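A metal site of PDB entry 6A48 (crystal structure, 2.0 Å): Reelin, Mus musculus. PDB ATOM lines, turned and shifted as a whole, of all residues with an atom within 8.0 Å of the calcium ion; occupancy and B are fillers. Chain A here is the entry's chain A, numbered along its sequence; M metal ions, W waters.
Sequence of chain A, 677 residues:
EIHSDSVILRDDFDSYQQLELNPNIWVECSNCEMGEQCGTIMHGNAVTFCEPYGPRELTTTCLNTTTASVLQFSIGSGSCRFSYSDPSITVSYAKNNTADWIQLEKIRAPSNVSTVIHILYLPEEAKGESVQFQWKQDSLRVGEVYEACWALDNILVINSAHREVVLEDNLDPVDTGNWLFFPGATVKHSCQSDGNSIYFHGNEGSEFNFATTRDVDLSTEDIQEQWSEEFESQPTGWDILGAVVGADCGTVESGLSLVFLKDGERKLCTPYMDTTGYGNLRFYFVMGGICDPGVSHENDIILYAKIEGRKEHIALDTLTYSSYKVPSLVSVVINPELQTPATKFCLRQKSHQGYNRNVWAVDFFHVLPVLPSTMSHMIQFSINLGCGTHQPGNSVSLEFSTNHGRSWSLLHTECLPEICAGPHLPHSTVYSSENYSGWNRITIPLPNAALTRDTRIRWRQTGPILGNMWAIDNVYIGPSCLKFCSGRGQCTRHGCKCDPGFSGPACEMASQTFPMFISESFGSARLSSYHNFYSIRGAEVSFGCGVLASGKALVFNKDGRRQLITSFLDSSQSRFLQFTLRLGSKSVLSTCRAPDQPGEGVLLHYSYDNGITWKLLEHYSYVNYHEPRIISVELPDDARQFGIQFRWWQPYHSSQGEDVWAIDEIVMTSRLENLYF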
ATOM      1  N   ASP A  11       5.881  -1.937 -15.365  1.00  0.00           N
ATOM      2  CA  ASP A  11       4.661  -1.149 -15.463  1.00  0.00           C
ATOM      3  C   ASP A  11       3.900  -1.259 -14.154  1.00  0.00           C
ATOM      4  O   ASP A  11       3.458  -2.352 -13.792  1.00  0.00           O
ATOM      5  CB  ASP A  11       3.803  -1.604 -16.643  1.00  0.00           C
ATOM      6  CG  ASP A  11       2.839  -0.533 -17.102  1.00  0.00           C
ATOM      7  OD1 ASP A  11       2.663   0.472 -16.380  1.00  0.00           O
ATOM      8  OD2 ASP A  11       2.259  -0.696 -18.200  1.00  0.00           O
ATOM      9  N   ASP A  12       3.764  -0.136 -13.453  1.00  0.00           N
ATOM     10  CA  ASP A  12       2.883  -0.047 -12.300  1.00  0.00           C
ATOM     11  C   ASP A  12       1.470   0.378 -12.682  1.00  0.00           C
ATOM     12  O   ASP A  12       0.617   0.489 -11.799  1.00  0.00           O
ATOM     13  CB  ASP A  12       3.461   0.924 -11.256  1.00  0.00           C
ATOM     14  CG  ASP A  12       3.679   2.335 -11.801  1.00  0.00           C
ATOM     15  OD1 ASP A  12       3.249   2.638 -12.944  1.00  0.00           O
ATOM     16  OD2 ASP A  12       4.293   3.155 -11.079  1.00  0.00           O
ATOM     17  N   PHE A  13       1.237   0.629 -13.967  1.00  0.00           N
ATOM     18  CA  PHE A  13      -0.044   1.053 -14.532  1.00  0.00           C
ATOM     19  C   PHE A  13      -0.481   2.425 -14.038  1.00  0.00           C
ATOM     20  O   PHE A  13      -1.635   2.825 -14.246  1.00  0.00           O
ATOM     21  CB  PHE A  13      -1.137   0.004 -14.281  1.00  0.00           C
ATOM     22  CG  PHE A  13      -0.760  -1.379 -14.731  1.00  0.00           C
ATOM     23  CD1 PHE A  13      -0.525  -1.642 -16.078  1.00  0.00           C
ATOM     24  CD2 PHE A  13      -0.604  -2.410 -13.822  1.00  0.00           C
ATOM     25  CE1 PHE A  13      -0.172  -2.907 -16.500  1.00  0.00           C
ATOM     26  CE2 PHE A  13      -0.245  -3.682 -14.241  1.00  0.00           C
ATOM     27  CZ  PHE A  13      -0.022  -3.926 -15.585  1.00  0.00           C
ATOM     28  N   ASP A  14       0.427   3.164 -13.402  1.00  0.00           N
ATOM     29  CA  ASP A  14       0.174   4.540 -12.985  1.00  0.00           C
ATOM     30  C   ASP A  14       1.130   5.513 -13.673  1.00  0.00           C
ATOM     31  O   ASP A  14       1.253   6.664 -13.249  1.00  0.00           O
ATOM     32  CB  ASP A  14       0.299   4.658 -11.462  1.00  0.00           C
ATOM     33  CG  ASP A  14      -0.685   3.762 -10.732  1.00  0.00           C
ATOM     34  OD1 ASP A  14      -1.895   4.024 -10.818  1.00  0.00           O
ATOM     35  OD2 ASP A  14      -0.238   2.806 -10.063  1.00  0.00           O
ATOM     36  N   SER A  15       1.802   5.067 -14.729  1.00  0.00           N
ATOM     37  CA  SER A  15       2.822   5.857 -15.413  1.00  0.00           C
ATOM     38  C   SER A  15       2.415   6.248 -16.830  1.00  0.00           C
ATOM     39  O   SER A  15       3.212   6.847 -17.552  1.00  0.00           O
ATOM     40  CB  SER A  15       4.148   5.091 -15.448  1.00  0.00           C
ATOM     41  OG  SER A  15       4.380   4.425 -14.218  1.00  0.00           O
ATOM     42  N   MET A  34      -8.275  -0.727 -16.711  1.00  0.00           N
ATOM     43  CA  MET A  34      -7.107  -0.175 -16.016  1.00  0.00           C
ATOM     44  C   MET A  34      -7.617   0.951 -15.116  1.00  0.00           C
ATOM     45  O   MET A  34      -7.932   2.043 -15.587  1.00  0.00           O
ATOM     46  CB  MET A  34      -6.050   0.328 -16.998  1.00  0.00           C
ATOM     47  CG  MET A  34      -4.765   0.777 -16.302  1.00  0.00           C
ATOM     48  SD  MET A  34      -3.470   1.373 -17.417  1.00  0.00           S
ATOM     49  CE  MET A  34      -3.950   3.084 -17.611  1.00  0.00           C
ATOM     50  N   GLY A  35      -7.688   0.670 -13.817  1.00  0.00           N
ATOM     51  CA  GLY A  35      -8.180   1.645 -12.864  1.00  0.00           C
ATOM     52  C   GLY A  35      -8.312   1.098 -11.460  1.00  0.00           C
ATOM     53  O   GLY A  35      -7.512   0.260 -11.037  1.00  0.00           O
ATOM     54  N   GLY A  39     -10.132  -1.366  -5.942  1.00  0.00           N
ATOM     55  CA  GLY A  39      -9.342  -0.671  -4.942  1.00  0.00           C
ATOM     56  C   GLY A  39      -7.852  -0.827  -5.208  1.00  0.00           C
ATOM     57  O   GLY A  39      -7.404  -1.070  -6.339  1.00  0.00           O
ATOM     58  N   THR A  40      -7.084  -0.693  -4.133  1.00  0.00           N
ATOM     59  CA  THR A  40      -5.629  -0.743  -4.230  1.00  0.00           C
ATOM     60  C   THR A  40      -5.143  -2.189  -4.224  1.00  0.00           C
ATOM     61  O   THR A  40      -5.543  -2.986  -3.372  1.00  0.00           O
ATOM     62  CB  THR A  40      -4.994   0.046  -3.087  1.00  0.00           C
ATOM     63  OG1 THR A  40      -5.359   1.423  -3.197  1.00  0.00           O
ATOM     64  CG2 THR A  40      -3.475  -0.080  -3.128  1.00  0.00           C
ATOM     65  N   ILE A  41      -4.288  -2.522  -5.198  1.00  0.00           N
ATOM     66  CA  ILE A  41      -3.597  -3.801  -5.208  1.00  0.00           C
ATOM     67  C   ILE A  41      -2.223  -3.569  -4.613  1.00  0.00           C
ATOM     68  O   ILE A  41      -1.948  -3.951  -3.471  1.00  0.00           O
ATOM     69  CB  ILE A  41      -3.534  -4.381  -6.632  1.00  0.00           C
ATOM     70  CG1 ILE A  41      -4.946  -4.552  -7.197  1.00  0.00           C
ATOM     71  CG2 ILE A  41      -2.807  -5.711  -6.643  1.00  0.00           C
ATOM     72  CD1 ILE A  41      -5.833  -5.437  -6.351  1.00  0.00           C
ATOM     73  N   MET A  42      -1.353  -2.913  -5.373  1.00  0.00           N
ATOM     74  CA  MET A  42      -0.120  -2.337  -4.851  1.00  0.00           C
ATOM     75  C   MET A  42      -0.275  -0.859  -4.531  1.00  0.00           C
ATOM     76  O   MET A  42      -0.017  -0.422  -3.412  1.00  0.00           O
ATOM     77  CB  MET A  42       1.028  -2.539  -5.850  1.00  0.00           C
ATOM     78  CG  MET A  42       1.510  -3.959  -5.990  1.00  0.00           C
ATOM     79  SD  MET A  42       2.406  -4.514  -4.544  1.00  0.00           S
ATOM     80  CE  MET A  42       1.203  -5.562  -3.804  1.00  0.00           C
ATOM     81  N   HIS A  43      -0.731  -0.083  -5.517  1.00  0.00           N
ATOM     82  CA  HIS A  43      -0.962   1.346  -5.389  1.00  0.00           C
ATOM     83  C   HIS A  43      -1.609   1.848  -6.666  1.00  0.00           C
ATOM     84  O   HIS A  43      -1.340   1.316  -7.748  1.00  0.00           O
ATOM     85  CB  HIS A  43       0.343   2.112  -5.119  1.00  0.00           C
ATOM     86  CG  HIS A  43       0.148   3.581  -4.976  1.00  0.00           C
ATOM     87  ND1 HIS A  43       0.483   4.477  -5.970  1.00  0.00           N
ATOM     88  CD2 HIS A  43      -0.372   4.318  -3.966  1.00  0.00           C
ATOM     89  CE1 HIS A  43       0.186   5.701  -5.571  1.00  0.00           C
ATOM     90  NE2 HIS A  43      -0.333   5.629  -4.362  1.00  0.00           N
ATOM     91  N   GLY A  44      -2.451   2.866  -6.534  1.00  0.00           N
ATOM     92  CA  GLY A  44      -3.022   3.515  -7.704  1.00  0.00           C
ATOM     93  C   GLY A  44      -3.830   2.546  -8.543  1.00  0.00           C
ATOM     94  O   GLY A  44      -4.675   1.801  -8.032  1.00  0.00           O
ATOM     95  N   ASN A  45      -3.563   2.551  -9.847  1.00  0.00           N
ATOM     96  CA  ASN A  45      -4.323   1.744 -10.796  1.00  0.00           C
ATOM     97  C   ASN A  45      -3.815   0.304 -10.835  1.00  0.00           C
ATOM     98  O   ASN A  45      -2.665   0.020 -10.506  1.00  0.00           O
ATOM     99  CB  ASN A  45      -4.258   2.341 -12.204  1.00  0.00           C
ATOM    100  CG  ASN A  45      -4.807   3.745 -12.266  1.00  0.00           C
ATOM    101  OD1 ASN A  45      -5.814   4.058 -11.629  1.00  0.00           O
ATOM    102  ND2 ASN A  45      -4.159   4.600 -13.041  1.00  0.00           N
ATOM    103  N   ALA A  46      -4.698  -0.590 -11.262  1.00  0.00           N
ATOM    104  CA  ALA A  46      -4.373  -1.977 -11.519  1.00  0.00           C
ATOM    105  C   ALA A  46      -5.139  -2.436 -12.753  1.00  0.00           C
ATOM    106  O   ALA A  46      -6.065  -1.766 -13.213  1.00  0.00           O
ATOM    107  CB  ALA A  46      -4.707  -2.878 -10.320  1.00  0.00           C
ATOM    108  N   VAL A  47      -4.740  -3.578 -13.309  1.00  0.00           N
ATOM    109  CA  VAL A  47      -5.451  -4.208 -14.414  1.00  0.00           C
ATOM    110  C   VAL A  47      -6.448  -5.182 -13.812  1.00  0.00           C
ATOM    111  O   VAL A  47      -6.064  -6.218 -13.259  1.00  0.00           O
ATOM    112  CB  VAL A  47      -4.496  -4.910 -15.385  1.00  0.00           C
ATOM    113  CG1 VAL A  47      -5.288  -5.617 -16.485  1.00  0.00           C
ATOM    114  CG2 VAL A  47      -3.526  -3.920 -15.991  1.00  0.00           C
ATOM    115  N   LEU A 152      -4.124  -7.360 -11.550  1.00  0.00           N
ATOM    116  CA  LEU A 152      -2.667  -7.371 -11.623  1.00  0.00           C
ATOM    117  C   LEU A 152      -2.099  -5.978 -11.362  1.00  0.00           C
ATOM    118  O   LEU A 152      -2.719  -4.965 -11.681  1.00  0.00           O
ATOM    119  CB  LEU A 152      -2.203  -7.843 -12.999  1.00  0.00           C
ATOM    120  CG  LEU A 152      -2.389  -9.323 -13.326  1.00  0.00           C
ATOM    121  CD1 LEU A 152      -2.242  -9.542 -14.824  1.00  0.00           C
ATOM    122  CD2 LEU A 152      -1.389 -10.164 -12.563  1.00  0.00           C
ATOM    123  N   ASP A 153      -0.897  -5.950 -10.783  1.00  0.00           N
ATOM    124  CA  ASP A 153      -0.220  -4.689 -10.500  1.00  0.00           C
ATOM    125  C   ASP A 153       1.278  -4.943 -10.373  1.00  0.00           C
ATOM    126  O   ASP A 153       1.698  -6.034  -9.974  1.00  0.00           O
ATOM    127  CB  ASP A 153      -0.755  -4.046  -9.214  1.00  0.00           C
ATOM    128  CG  ASP A 153      -0.581  -2.537  -9.188  1.00  0.00           C
ATOM    129  OD1 ASP A 153       0.067  -1.989 -10.108  1.00  0.00           O
ATOM    130  OD2 ASP A 153      -1.095  -1.908  -8.244  1.00  0.00           O
ATOM    131  N   ASN A 154       2.076  -3.938 -10.736  1.00  0.00           N
ATOM    132  CA  ASN A 154       3.531  -3.943 -10.573  1.00  0.00           C
ATOM    133  C   ASN A 154       4.159  -5.193 -11.196  1.00  0.00           C
ATOM    134  O   ASN A 154       4.642  -6.097 -10.520  1.00  0.00           O
ATOM    135  CB  ASN A 154       3.909  -3.838  -9.085  1.00  0.00           C
ATOM    136  CG  ASN A 154       3.772  -2.415  -8.545  1.00  0.00           C
ATOM    137  OD1 ASN A 154       3.238  -1.529  -9.211  1.00  0.00           O
ATOM    138  ND2 ASN A 154       4.261  -2.206  -7.324  1.00  0.00           N
ATOM    139  N   ILE A 155       4.170  -5.200 -12.520  1.00  0.00           N
ATOM    140  CA  ILE A 155       4.735  -6.299 -13.306  1.00  0.00           C
ATOM    141  C   ILE A 155       6.156  -5.921 -13.706  1.00  0.00           C
ATOM    142  O   ILE A 155       6.411  -4.809 -14.182  1.00  0.00           O
ATOM    143  CB  ILE A 155       3.867  -6.617 -14.520  1.00  0.00           C
ATOM    144  CG1 ILE A 155       2.465  -7.036 -14.051  1.00  0.00           C
ATOM    145  CG2 ILE A 155       4.510  -7.711 -15.374  1.00  0.00           C
ATOM    146  CD1 ILE A 155       1.471  -7.274 -15.156  1.00  0.00           C
ATOM    147  N   PHE A 181      10.208  -0.800  -7.651  1.00  0.00           N
ATOM    148  CA  PHE A 181       8.987  -0.046  -7.429  1.00  0.00           C
ATOM    149  C   PHE A 181       9.086   0.681  -6.106  1.00  0.00           C
ATOM    150  O   PHE A 181       9.828   0.280  -5.211  1.00  0.00           O
ATOM    151  CB  PHE A 181       7.730  -0.927  -7.412  1.00  0.00           C
ATOM    152  CG  PHE A 181       7.523  -1.743  -8.656  1.00  0.00           C
ATOM    153  CD1 PHE A 181       7.025  -1.162  -9.812  1.00  0.00           C
ATOM    154  CD2 PHE A 181       7.774  -3.112  -8.646  1.00  0.00           C
ATOM    155  CE1 PHE A 181       6.820  -1.921 -10.948  1.00  0.00           C
ATOM    156  CE2 PHE A 181       7.561  -3.875  -9.778  1.00  0.00           C
ATOM    157  CZ  PHE A 181       7.080  -3.279 -10.935  1.00  0.00           C
ATOM    158  N   PRO A 183       5.787   1.663  -4.209  1.00  0.00           N
ATOM    159  CA  PRO A 183       4.345   1.866  -4.053  1.00  0.00           C
ATOM    160  C   PRO A 183       4.028   2.833  -2.930  1.00  0.00           C
ATOM    161  O   PRO A 183       4.527   2.720  -1.812  1.00  0.00           O
ATOM    162  CB  PRO A 183       3.813   0.456  -3.751  1.00  0.00           C
ATOM    163  CG  PRO A 183       5.005  -0.293  -3.229  1.00  0.00           C
ATOM    164  CD  PRO A 183       6.175   0.259  -3.968  1.00  0.00           C
HETATM  165 CA    CA M   1      -0.448   0.471  -9.729  1.00  0.00          CA
HETATM  166  O   HOH W   1       1.437   0.396  -8.316  1.00  0.00           O
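OD1 of Asp 12 is in hydrogen-bond range of OG of Ser 15. O of Phe 13 is in hydrogen-bond range of ND2 of Asn 45. The side-chain amide oxygen (OD1) of Asn 154 sits close to the side-chain carboxylate (OD1) of Asp 153 (3.3 Å). The backbone NH of Met 42 sits close to the side-chain carboxylate of Asp 153 (3.1 Å).
Five residues have an atom within 4 Å of the calcium ion: Asp 12, Asp 14, His 43, Asn 45 and Asp 153.
The calcium ion is bound by the backbone carbonyl oxygen (O) of Asp 12 (2.3 Å), the backbone carbonyl oxygen (O) of His 43 (2.3 Å), water W1 (2.4 Å), the side-chain carboxylate (OD2) of Asp 14 (2.4 Å), the backbone carbonyl oxygen (O) of Asn 45 (2.4 Å), the side-chain carboxylate (OD1) of Asp 153 (2.5 Å) and the side-chain carboxylate (OD2) of Asp 153 (2.9 Å).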
